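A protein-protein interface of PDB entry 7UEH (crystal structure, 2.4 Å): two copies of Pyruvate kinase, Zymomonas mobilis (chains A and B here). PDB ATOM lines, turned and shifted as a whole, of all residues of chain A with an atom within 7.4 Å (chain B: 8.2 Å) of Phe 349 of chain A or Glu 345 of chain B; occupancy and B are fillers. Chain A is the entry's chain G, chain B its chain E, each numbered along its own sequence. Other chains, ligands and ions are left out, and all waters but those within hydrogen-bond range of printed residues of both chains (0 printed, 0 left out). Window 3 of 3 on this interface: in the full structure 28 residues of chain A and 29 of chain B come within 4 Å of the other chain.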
ATOM      1  N   GLU A 267     -19.304  24.721  14.289  1.00  0.00           N
ATOM      2  CA  GLU A 267     -20.419  24.935  15.219  1.00  0.00           C
ATOM      3  C   GLU A 267     -19.993  25.785  16.410  1.00  0.00           C
ATOM      4  O   GLU A 267     -20.625  26.795  16.723  1.00  0.00           O
ATOM      5  CB  GLU A 267     -20.953  23.605  15.749  1.00  0.00           C
ATOM      6  CG  GLU A 267     -21.642  22.778  14.731  1.00  0.00           C
ATOM      7  CD  GLU A 267     -21.908  21.358  15.218  1.00  0.00           C
ATOM      8  OE1 GLU A 267     -21.363  20.966  16.299  1.00  0.00           O
ATOM      9  OE2 GLU A 267     -22.648  20.651  14.489  1.00  0.00           O
ATOM     10  N   ARG A 270     -19.174  29.472  15.725  1.00  0.00           N
ATOM     11  CA  ARG A 270     -20.340  30.325  15.554  1.00  0.00           C
ATOM     12  C   ARG A 270     -21.015  30.595  16.884  1.00  0.00           C
ATOM     13  O   ARG A 270     -21.422  31.739  17.167  1.00  0.00           O
ATOM     14  CB  ARG A 270     -21.338  29.691  14.588  1.00  0.00           C
ATOM     15  CG  ARG A 270     -20.959  29.788  13.153  1.00  0.00           C
ATOM     16  CD  ARG A 270     -21.954  29.023  12.247  1.00  0.00           C
ATOM     17  NE  ARG A 270     -23.293  29.553  12.313  1.00  0.00           N
ATOM     18  CZ  ARG A 270     -24.363  29.049  11.695  1.00  0.00           C
ATOM     19  NH1 ARG A 270     -24.292  27.960  10.926  1.00  0.00           N
ATOM     20  NH2 ARG A 270     -25.535  29.646  11.877  1.00  0.00           N
ATOM     21  N   GLN A 271     -21.169  29.558  17.714  1.00  0.00           N
ATOM     22  CA  GLN A 271     -21.906  29.766  18.956  1.00  0.00           C
ATOM     23  C   GLN A 271     -21.140  30.690  19.887  1.00  0.00           C
ATOM     24  O   GLN A 271     -21.751  31.405  20.686  1.00  0.00           O
ATOM     25  CB  GLN A 271     -22.186  28.445  19.655  1.00  0.00           C
ATOM     26  CG  GLN A 271     -22.799  27.427  18.740  1.00  0.00           C
ATOM     27  CD  GLN A 271     -22.956  26.078  19.372  1.00  0.00           C
ATOM     28  OE1 GLN A 271     -22.054  25.559  20.017  1.00  0.00           O
ATOM     29  NE2 GLN A 271     -24.116  25.503  19.194  1.00  0.00           N
ATOM     30  N   TYR A 305     -22.631  26.074   3.727  1.00  0.00           N
ATOM     31  CA  TYR A 305     -23.864  25.598   4.358  1.00  0.00           C
ATOM     32  C   TYR A 305     -23.685  25.359   5.858  1.00  0.00           C
ATOM     33  O   TYR A 305     -24.666  25.386   6.608  1.00  0.00           O
ATOM     34  CB  TYR A 305     -24.362  24.288   3.728  1.00  0.00           C
ATOM     35  CG  TYR A 305     -25.037  24.351   2.374  1.00  0.00           C
ATOM     36  CD1 TYR A 305     -26.080  25.219   2.108  1.00  0.00           C
ATOM     37  CD2 TYR A 305     -24.639  23.488   1.356  1.00  0.00           C
ATOM     38  CE1 TYR A 305     -26.689  25.238   0.863  1.00  0.00           C
ATOM     39  CE2 TYR A 305     -25.227  23.509   0.114  1.00  0.00           C
ATOM     40  CZ  TYR A 305     -26.248  24.372  -0.145  1.00  0.00           C
ATOM     41  OH  TYR A 305     -26.805  24.336  -1.437  1.00  0.00           O
ATOM     42  N   TYR A 343     -30.340  27.065   1.461  1.00  0.00           N
ATOM     43  CA  TYR A 343     -29.170  27.640   2.123  1.00  0.00           C
ATOM     44  C   TYR A 343     -29.467  28.050   3.562  1.00  0.00           C
ATOM     45  O   TYR A 343     -28.804  27.593   4.499  1.00  0.00           O
ATOM     46  CB  TYR A 343     -28.645  28.833   1.322  1.00  0.00           C
ATOM     47  CG  TYR A 343     -27.708  29.732   2.106  1.00  0.00           C
ATOM     48  CD1 TYR A 343     -26.398  29.353   2.352  1.00  0.00           C
ATOM     49  CD2 TYR A 343     -28.141  30.940   2.626  1.00  0.00           C
ATOM     50  CE1 TYR A 343     -25.542  30.142   3.066  1.00  0.00           C
ATOM     51  CE2 TYR A 343     -27.286  31.753   3.357  1.00  0.00           C
ATOM     52  CZ  TYR A 343     -25.978  31.342   3.567  1.00  0.00           C
ATOM     53  OH  TYR A 343     -25.094  32.118   4.251  1.00  0.00           O
ATOM     54  N   ILE A 344     -30.456  28.920   3.781  1.00  0.00           N
ATOM     55  CA  ILE A 344     -30.651  29.446   5.140  1.00  0.00           C
ATOM     56  C   ILE A 344     -31.039  28.319   6.099  1.00  0.00           C
ATOM     57  O   ILE A 344     -30.608  28.293   7.256  1.00  0.00           O
ATOM     58  CB  ILE A 344     -31.636  30.643   5.129  1.00  0.00           C
ATOM     59  CG1 ILE A 344     -31.577  31.469   6.420  1.00  0.00           C
ATOM     60  CG2 ILE A 344     -33.091  30.263   4.830  1.00  0.00           C
ATOM     61  CD1 ILE A 344     -30.108  31.933   6.817  1.00  0.00           C
ATOM     62  N   GLU A 345     -31.814  27.343   5.630  1.00  0.00           N
ATOM     63  CA  GLU A 345     -32.168  26.233   6.512  1.00  0.00           C
ATOM     64  C   GLU A 345     -30.942  25.475   7.001  1.00  0.00           C
ATOM     65  O   GLU A 345     -30.895  25.027   8.148  1.00  0.00           O
ATOM     66  CB  GLU A 345     -33.117  25.275   5.815  1.00  0.00           C
ATOM     67  CG  GLU A 345     -34.442  25.937   5.459  1.00  0.00           C
ATOM     68  CD  GLU A 345     -34.428  26.590   4.071  1.00  0.00           C
ATOM     69  OE1 GLU A 345     -33.319  26.774   3.514  1.00  0.00           O
ATOM     70  OE2 GLU A 345     -35.523  26.901   3.543  1.00  0.00           O
ATOM     71  N   ARG A 346     -29.945  25.299   6.153  1.00  0.00           N
ATOM     72  CA  ARG A 346     -28.779  24.569   6.619  1.00  0.00           C
ATOM     73  C   ARG A 346     -27.956  25.405   7.578  1.00  0.00           C
ATOM     74  O   ARG A 346     -27.449  24.886   8.576  1.00  0.00           O
ATOM     75  CB  ARG A 346     -27.980  24.101   5.426  1.00  0.00           C
ATOM     76  CG  ARG A 346     -28.573  22.812   4.905  1.00  0.00           C
ATOM     77  CD  ARG A 346     -28.296  22.568   3.444  1.00  0.00           C
ATOM     78  NE  ARG A 346     -28.883  21.303   3.098  1.00  0.00           N
ATOM     79  CZ  ARG A 346     -30.068  21.166   2.544  1.00  0.00           C
ATOM     80  NH1 ARG A 346     -30.799  22.221   2.237  1.00  0.00           N
ATOM     81  NH2 ARG A 346     -30.513  19.960   2.298  1.00  0.00           N
ATOM     82  N   VAL A 347     -27.891  26.707   7.348  1.00  0.00           N
ATOM     83  CA  VAL A 347     -27.164  27.590   8.264  1.00  0.00           C
ATOM     84  C   VAL A 347     -27.826  27.579   9.632  1.00  0.00           C
ATOM     85  O   VAL A 347     -27.155  27.487  10.678  1.00  0.00           O
ATOM     86  CB  VAL A 347     -27.086  29.007   7.655  1.00  0.00           C
ATOM     87  CG1 VAL A 347     -26.623  30.080   8.665  1.00  0.00           C
ATOM     88  CG2 VAL A 347     -26.177  28.992   6.425  1.00  0.00           C
ATOM     89  N   ARG A 348     -29.155  27.624   9.647  1.00  0.00           N
ATOM     90  CA  ARG A 348     -29.913  27.727  10.892  1.00  0.00           C
ATOM     91  C   ARG A 348     -29.910  26.437  11.701  1.00  0.00           C
ATOM     92  O   ARG A 348     -30.366  26.445  12.834  1.00  0.00           O
ATOM     93  CB  ARG A 348     -31.361  28.105  10.593  1.00  0.00           C
ATOM     94  CG  ARG A 348     -31.586  29.481  10.056  1.00  0.00           C
ATOM     95  CD  ARG A 348     -32.046  30.467  11.079  1.00  0.00           C
ATOM     96  NE  ARG A 348     -32.336  31.747  10.436  1.00  0.00           N
ATOM     97  CZ  ARG A 348     -31.431  32.686  10.232  1.00  0.00           C
ATOM     98  NH1 ARG A 348     -30.189  32.487  10.620  1.00  0.00           N
ATOM     99  NH2 ARG A 348     -31.753  33.807   9.615  1.00  0.00           N
ATOM    100  N   PHE A 349     -29.428  25.335  11.142  1.00  0.00           N
ATOM    101  CA  PHE A 349     -29.311  24.102  11.907  1.00  0.00           C
ATOM    102  C   PHE A 349     -28.415  24.253  13.108  1.00  0.00           C
ATOM    103  O   PHE A 349     -28.559  23.508  14.070  1.00  0.00           O
ATOM    104  CB  PHE A 349     -28.776  23.029  10.991  1.00  0.00           C
ATOM    105  CG  PHE A 349     -28.557  21.706  11.617  1.00  0.00           C
ATOM    106  CD1 PHE A 349     -29.614  20.828  11.796  1.00  0.00           C
ATOM    107  CD2 PHE A 349     -27.277  21.282  11.902  1.00  0.00           C
ATOM    108  CE1 PHE A 349     -29.399  19.592  12.287  1.00  0.00           C
ATOM    109  CE2 PHE A 349     -27.045  20.011  12.417  1.00  0.00           C
ATOM    110  CZ  PHE A 349     -28.107  19.169  12.598  1.00  0.00           C
ATOM    111  N   THR A 350     -27.465  25.171  13.072  1.00  0.00           N
ATOM    112  CA  THR A 350     -26.637  25.398  14.247  1.00  0.00           C
ATOM    113  C   THR A 350     -27.282  26.476  15.091  1.00  0.00           C
ATOM    114  O   THR A 350     -27.332  27.633  14.655  1.00  0.00           O
ATOM    115  CB  THR A 350     -25.231  25.829  13.887  1.00  0.00           C
ATOM    116  OG1 THR A 350     -24.606  24.858  13.045  1.00  0.00           O
ATOM    117  CG2 THR A 350     -24.452  26.006  15.201  1.00  0.00           C
ATOM    118  N   PRO A 351     -27.734  26.176  16.298  1.00  0.00           N
ATOM    119  CA  PRO A 351     -28.375  27.204  17.109  1.00  0.00           C
ATOM    120  C   PRO A 351     -27.312  28.155  17.641  1.00  0.00           C
ATOM    121  O   PRO A 351     -26.193  27.737  17.932  1.00  0.00           O
ATOM    122  CB  PRO A 351     -29.046  26.394  18.216  1.00  0.00           C
ATOM    123  CG  PRO A 351     -28.173  25.158  18.346  1.00  0.00           C
ATOM    124  CD  PRO A 351     -27.553  24.904  17.038  1.00  0.00           C
ATOM    125  N   THR A 352     -27.655  29.448  17.714  1.00  0.00           N
ATOM    126  CA  THR A 352     -26.755  30.488  18.216  1.00  0.00           C
ATOM    127  C   THR A 352     -27.575  31.418  19.101  1.00  0.00           C
ATOM    128  O   THR A 352     -27.848  32.577  18.757  1.00  0.00           O
ATOM    129  CB  THR A 352     -26.057  31.254  17.078  1.00  0.00           C
ATOM    130  OG1 THR A 352     -27.009  31.956  16.284  1.00  0.00           O
ATOM    131  CG2 THR A 352     -25.290  30.323  16.182  1.00  0.00           C
ATOM    132  N   ARG B 270     -34.910  10.627  -0.606  1.00  0.00           N
ATOM    133  CA  ARG B 270     -35.180  10.028   0.713  1.00  0.00           C
ATOM    134  C   ARG B 270     -36.648  10.110   1.060  1.00  0.00           C
ATOM    135  O   ARG B 270     -37.247   9.132   1.502  1.00  0.00           O
ATOM    136  CB  ARG B 270     -34.350  10.715   1.796  1.00  0.00           C
ATOM    137  CG  ARG B 270     -32.904  10.286   1.842  1.00  0.00           C
ATOM    138  CD  ARG B 270     -32.170  10.933   2.978  1.00  0.00           C
ATOM    139  NE  ARG B 270     -32.851  10.723   4.235  1.00  0.00           N
ATOM    140  CZ  ARG B 270     -32.587  11.396   5.342  1.00  0.00           C
ATOM    141  NH1 ARG B 270     -31.604  12.291   5.362  1.00  0.00           N
ATOM    142  NH2 ARG B 270     -33.326  11.166   6.425  1.00  0.00           N
ATOM    143  N   TYR B 305     -23.755  12.545   5.467  1.00  0.00           N
ATOM    144  CA  TYR B 305     -24.555  13.402   6.336  1.00  0.00           C
ATOM    145  C   TYR B 305     -25.882  13.810   5.696  1.00  0.00           C
ATOM    146  O   TYR B 305     -26.857  14.036   6.404  1.00  0.00           O
ATOM    147  CB  TYR B 305     -23.788  14.677   6.702  1.00  0.00           C
ATOM    148  CG  TYR B 305     -22.644  14.526   7.664  1.00  0.00           C
ATOM    149  CD1 TYR B 305     -22.805  13.886   8.895  1.00  0.00           C
ATOM    150  CD2 TYR B 305     -21.404  15.052   7.366  1.00  0.00           C
ATOM    151  CE1 TYR B 305     -21.744  13.754   9.778  1.00  0.00           C
ATOM    152  CE2 TYR B 305     -20.337  14.918   8.244  1.00  0.00           C
ATOM    153  CZ  TYR B 305     -20.506  14.260   9.448  1.00  0.00           C
ATOM    154  OH  TYR B 305     -19.433  14.143  10.330  1.00  0.00           O
ATOM    155  N   ALA B 340     -19.135   8.724  14.327  1.00  0.00           N
ATOM    156  CA  ALA B 340     -18.643   9.918  15.014  1.00  0.00           C
ATOM    157  C   ALA B 340     -19.812  10.807  15.450  1.00  0.00           C
ATOM    158  O   ALA B 340     -20.929  10.661  14.954  1.00  0.00           O
ATOM    159  CB  ALA B 340     -17.700  10.693  14.082  1.00  0.00           C
ATOM    160  N   PRO B 341     -19.620  11.744  16.368  1.00  0.00           N
ATOM    161  CA  PRO B 341     -20.748  12.608  16.753  1.00  0.00           C
ATOM    162  C   PRO B 341     -21.193  13.502  15.617  1.00  0.00           C
ATOM    163  O   PRO B 341     -20.406  13.877  14.744  1.00  0.00           O
ATOM    164  CB  PRO B 341     -20.194  13.449  17.905  1.00  0.00           C
ATOM    165  CG  PRO B 341     -19.195  12.560  18.517  1.00  0.00           C
ATOM    166  CD  PRO B 341     -18.507  11.883  17.314  1.00  0.00           C
ATOM    167  N   GLY B 342     -22.486  13.831  15.647  1.00  0.00           N
ATOM    168  CA  GLY B 342     -23.095  14.720  14.695  1.00  0.00           C
ATOM    169  C   GLY B 342     -23.692  14.041  13.479  1.00  0.00           C
ATOM    170  O   GLY B 342     -24.209  14.732  12.596  1.00  0.00           O
ATOM    171  N   TYR B 343     -23.647  12.718  13.406  1.00  0.00           N
ATOM    172  CA  TYR B 343     -24.145  12.038  12.225  1.00  0.00           C
ATOM    173  C   TYR B 343     -25.668  12.011  12.168  1.00  0.00           C
ATOM    174  O   TYR B 343     -26.256  12.546  11.225  1.00  0.00           O
ATOM    175  CB  TYR B 343     -23.592  10.627  12.187  1.00  0.00           C
ATOM    176  CG  TYR B 343     -24.298   9.738  11.248  1.00  0.00           C
ATOM    177  CD1 TYR B 343     -24.129   9.872   9.874  1.00  0.00           C
ATOM    178  CD2 TYR B 343     -25.144   8.766  11.717  1.00  0.00           C
ATOM    179  CE1 TYR B 343     -24.770   9.041   9.001  1.00  0.00           C
ATOM    180  CE2 TYR B 343     -25.792   7.951  10.857  1.00  0.00           C
ATOM    181  CZ  TYR B 343     -25.575   8.080   9.489  1.00  0.00           C
ATOM    182  OH  TYR B 343     -26.199   7.268   8.611  1.00  0.00           O
ATOM    183  N   ILE B 344     -26.322  11.408  13.172  1.00  0.00           N
ATOM    184  CA  ILE B 344     -27.749  11.171  13.053  1.00  0.00           C
ATOM    185  C   ILE B 344     -28.511  12.490  13.061  1.00  0.00           C
ATOM    186  O   ILE B 344     -29.520  12.625  12.361  1.00  0.00           O
ATOM    187  CB  ILE B 344     -28.250  10.194  14.133  1.00  0.00           C
ATOM    188  CG1 ILE B 344     -29.638   9.650  13.765  1.00  0.00           C
ATOM    189  CG2 ILE B 344     -28.275  10.822  15.508  1.00  0.00           C
ATOM    190  CD1 ILE B 344     -29.613   8.667  12.527  1.00  0.00           C
ATOM    191  N   GLU B 345     -28.033  13.483  13.807  1.00  0.00           N
ATOM    192  CA  GLU B 345     -28.680  14.797  13.810  1.00  0.00           C
ATOM    193  C   GLU B 345     -28.804  15.353  12.401  1.00  0.00           C
ATOM    194  O   GLU B 345     -29.856  15.888  12.012  1.00  0.00           O
ATOM    195  CB  GLU B 345     -27.892  15.787  14.662  1.00  0.00           C
ATOM    196  CG  GLU B 345     -27.894  15.486  16.116  1.00  0.00           C
ATOM    197  CD  GLU B 345     -26.837  14.463  16.484  1.00  0.00           C
ATOM    198  OE1 GLU B 345     -26.150  13.975  15.571  1.00  0.00           O
ATOM    199  OE2 GLU B 345     -26.704  14.182  17.691  1.00  0.00           O
ATOM    200  N   ARG B 346     -27.717  15.242  11.629  1.00  0.00           N
ATOM    201  CA  ARG B 346     -27.713  15.725  10.258  1.00  0.00           C
ATOM    202  C   ARG B 346     -28.560  14.843   9.360  1.00  0.00           C
ATOM    203  O   ARG B 346     -29.227  15.343   8.443  1.00  0.00           O
ATOM    204  CB  ARG B 346     -26.268  15.819   9.752  1.00  0.00           C
ATOM    205  CG  ARG B 346     -25.627  17.126  10.199  1.00  0.00           C
ATOM    206  CD  ARG B 346     -24.131  17.070  10.253  1.00  0.00           C
ATOM    207  NE  ARG B 346     -23.646  18.359  10.692  1.00  0.00           N
ATOM    208  CZ  ARG B 346     -23.322  18.661  11.943  1.00  0.00           C
ATOM    209  NH1 ARG B 346     -23.375  17.746  12.905  1.00  0.00           N
ATOM    210  NH2 ARG B 346     -22.926  19.888  12.211  1.00  0.00           N
ATOM    211  N   VAL B 347     -28.581  13.541   9.613  1.00  0.00           N
ATOM    212  CA  VAL B 347     -29.413  12.692   8.774  1.00  0.00           C
ATOM    213  C   VAL B 347     -30.880  13.044   9.007  1.00  0.00           C
ATOM    214  O   VAL B 347     -31.690  13.080   8.070  1.00  0.00           O
ATOM    215  CB  VAL B 347     -29.116  11.201   9.045  1.00  0.00           C
ATOM    216  CG1 VAL B 347     -30.113  10.370   8.303  1.00  0.00           C
ATOM    217  CG2 VAL B 347     -27.703  10.822   8.632  1.00  0.00           C
ATOM    218  N   ARG B 348     -31.220  13.370  10.258  1.00  0.00           N
ATOM    219  CA  ARG B 348     -32.588  13.649  10.669  1.00  0.00           C
ATOM    220  C   ARG B 348     -33.076  15.009  10.219  1.00  0.00           C
ATOM    221  O   ARG B 348     -34.279  15.261  10.309  1.00  0.00           O
ATOM    222  CB  ARG B 348     -32.699  13.517  12.190  1.00  0.00           C
ATOM    223  CG  ARG B 348     -32.527  12.068  12.653  1.00  0.00           C
ATOM    224  CD  ARG B 348     -33.821  11.377  12.895  1.00  0.00           C
ATOM    225  NE  ARG B 348     -33.559  10.095  13.510  1.00  0.00           N
ATOM    226  CZ  ARG B 348     -33.297   8.976  12.842  1.00  0.00           C
ATOM    227  NH1 ARG B 348     -33.276   8.957  11.501  1.00  0.00           N
ATOM    228  NH2 ARG B 348     -33.080   7.860  13.533  1.00  0.00           N
ATOM    229  N   PHE B 349     -32.176  15.865   9.720  1.00  0.00           N
ATOM    230  CA  PHE B 349     -32.569  17.147   9.155  1.00  0.00           C
ATOM    231  C   PHE B 349     -33.647  17.004   8.079  1.00  0.00           C
ATOM    232  O   PHE B 349     -34.444  17.921   7.874  1.00  0.00           O
ATOM    233  CB  PHE B 349     -31.306  17.819   8.588  1.00  0.00           C
ATOM    234  CG  PHE B 349     -31.534  19.168   7.997  1.00  0.00           C
ATOM    235  CD1 PHE B 349     -31.693  20.263   8.795  1.00  0.00           C
ATOM    236  CD2 PHE B 349     -31.531  19.343   6.624  1.00  0.00           C
ATOM    237  CE1 PHE B 349     -31.877  21.540   8.252  1.00  0.00           C
ATOM    238  CE2 PHE B 349     -31.722  20.623   6.051  1.00  0.00           C
ATOM    239  CZ  PHE B 349     -31.891  21.725   6.874  1.00  0.00           C
ATOM    240  N   THR B 350     -33.659  15.896   7.352  1.00  0.00           N
ATOM    241  CA  THR B 350     -34.575  15.710   6.232  1.00  0.00           C
ATOM    242  C   THR B 350     -35.789  14.942   6.745  1.00  0.00           C
ATOM    243  O   THR B 350     -35.645  13.775   7.143  1.00  0.00           O
ATOM    244  CB  THR B 350     -33.900  14.940   5.090  1.00  0.00           C
ATOM    245  OG1 THR B 350     -32.831  15.722   4.544  1.00  0.00           O
ATOM    246  CG2 THR B 350     -34.913  14.577   4.016  1.00  0.00           C
ATOM    247  N   VAL B 397     -31.561   4.047  13.874  1.00  0.00           N
ATOM    248  CA  VAL B 397     -30.279   3.908  14.536  1.00  0.00           C
ATOM    249  C   VAL B 397     -29.920   2.440  14.638  1.00  0.00           C
ATOM    250  O   VAL B 397     -28.820   2.015  14.250  1.00  0.00           O
ATOM    251  CB  VAL B 397     -30.335   4.555  15.924  1.00  0.00           C
ATOM    252  CG1 VAL B 397     -29.053   4.263  16.711  1.00  0.00           C
ATOM    253  CG2 VAL B 397     -30.571   6.066  15.839  1.00  0.00           C
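Printed residues of chain B that touch a printed residue of chain A: Glu 345, Arg 346 and Phe 349.
Hydrophobic or aromatic side chains of chain B that line the printed part of chain A: Phe 349.
Among the printed residues, 6 pairs touch across the chains.
Among the printed residues, Asp or Glu carboxylates within 4 Å of a Lys or Arg side-chain nitrogen of the other chain: Glu 267 of chain A with Arg 346 of chain B (2.4 Å).
NH1 of Arg 346 of chain B lies within hydrogen-bond range of O of Gly 342 of chain B (3.1 Å).
Printed residues of chain B within 4 Å of Glu 345 of chain A: Phe 349.
Phe 349 of chain A touches just these residues of chain B: Glu 345 (3.7 Å), Arg 346 (3.9 Å) and Phe 349 (3.7 Å).
Gly 342 of chain B touches none of the printed residues of chain A.
Glu 345 of chain B touches just one residue of chain A: Phe 349.
Printed residues of chain A within 4 Å of Arg 346 of chain B: Glu 267 (2.4 Å) and Phe 349 (3.9 Å).
Val 347 of chain B touches none of the printed residues of chain A.
The nearest residue of chain A that does not touch Glu 345 of chain B is Glu 267 of chain A (7.2 Å).
The nearest printed residue of chain A that does not touch Phe 349 of chain B is Arg 348 of chain A (6.3 Å).
NH2 of Arg 346 of chain B is in salt-bridge range of OE2 of Glu 267 of chain A (2.4 Å).
Glu 345 of chain A touches Phe 349 of chain B (O to CE1, 3.6 Å).
Phe 349 of chain B touches Arg 346 of chain A (CE2 to CZ, 3.9 Å).
Glu 345 of chain B touches Phe 349 of chain A (O to CE1, 3.7 Å).
Phe 349 of chain A touches Arg 346 of chain B (CE2 to CG, 3.9 Å).
CD1 of Phe 349 of chain A touches CD1 of Phe 349 of chain B, 3.7 Å away.
Glu 345 of chain A touches Phe 349 of chain B, and with the chains exchanged Phe 349 of chain A touches Glu 345 of chain B.
Arg 346 of chain A touches Phe 349 of chain B, and with the chains exchanged Phe 349 of chain A touches Arg 346 of chain B.
Phe 349 of chain B touches its own counterpart, Phe 349 of chain A.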
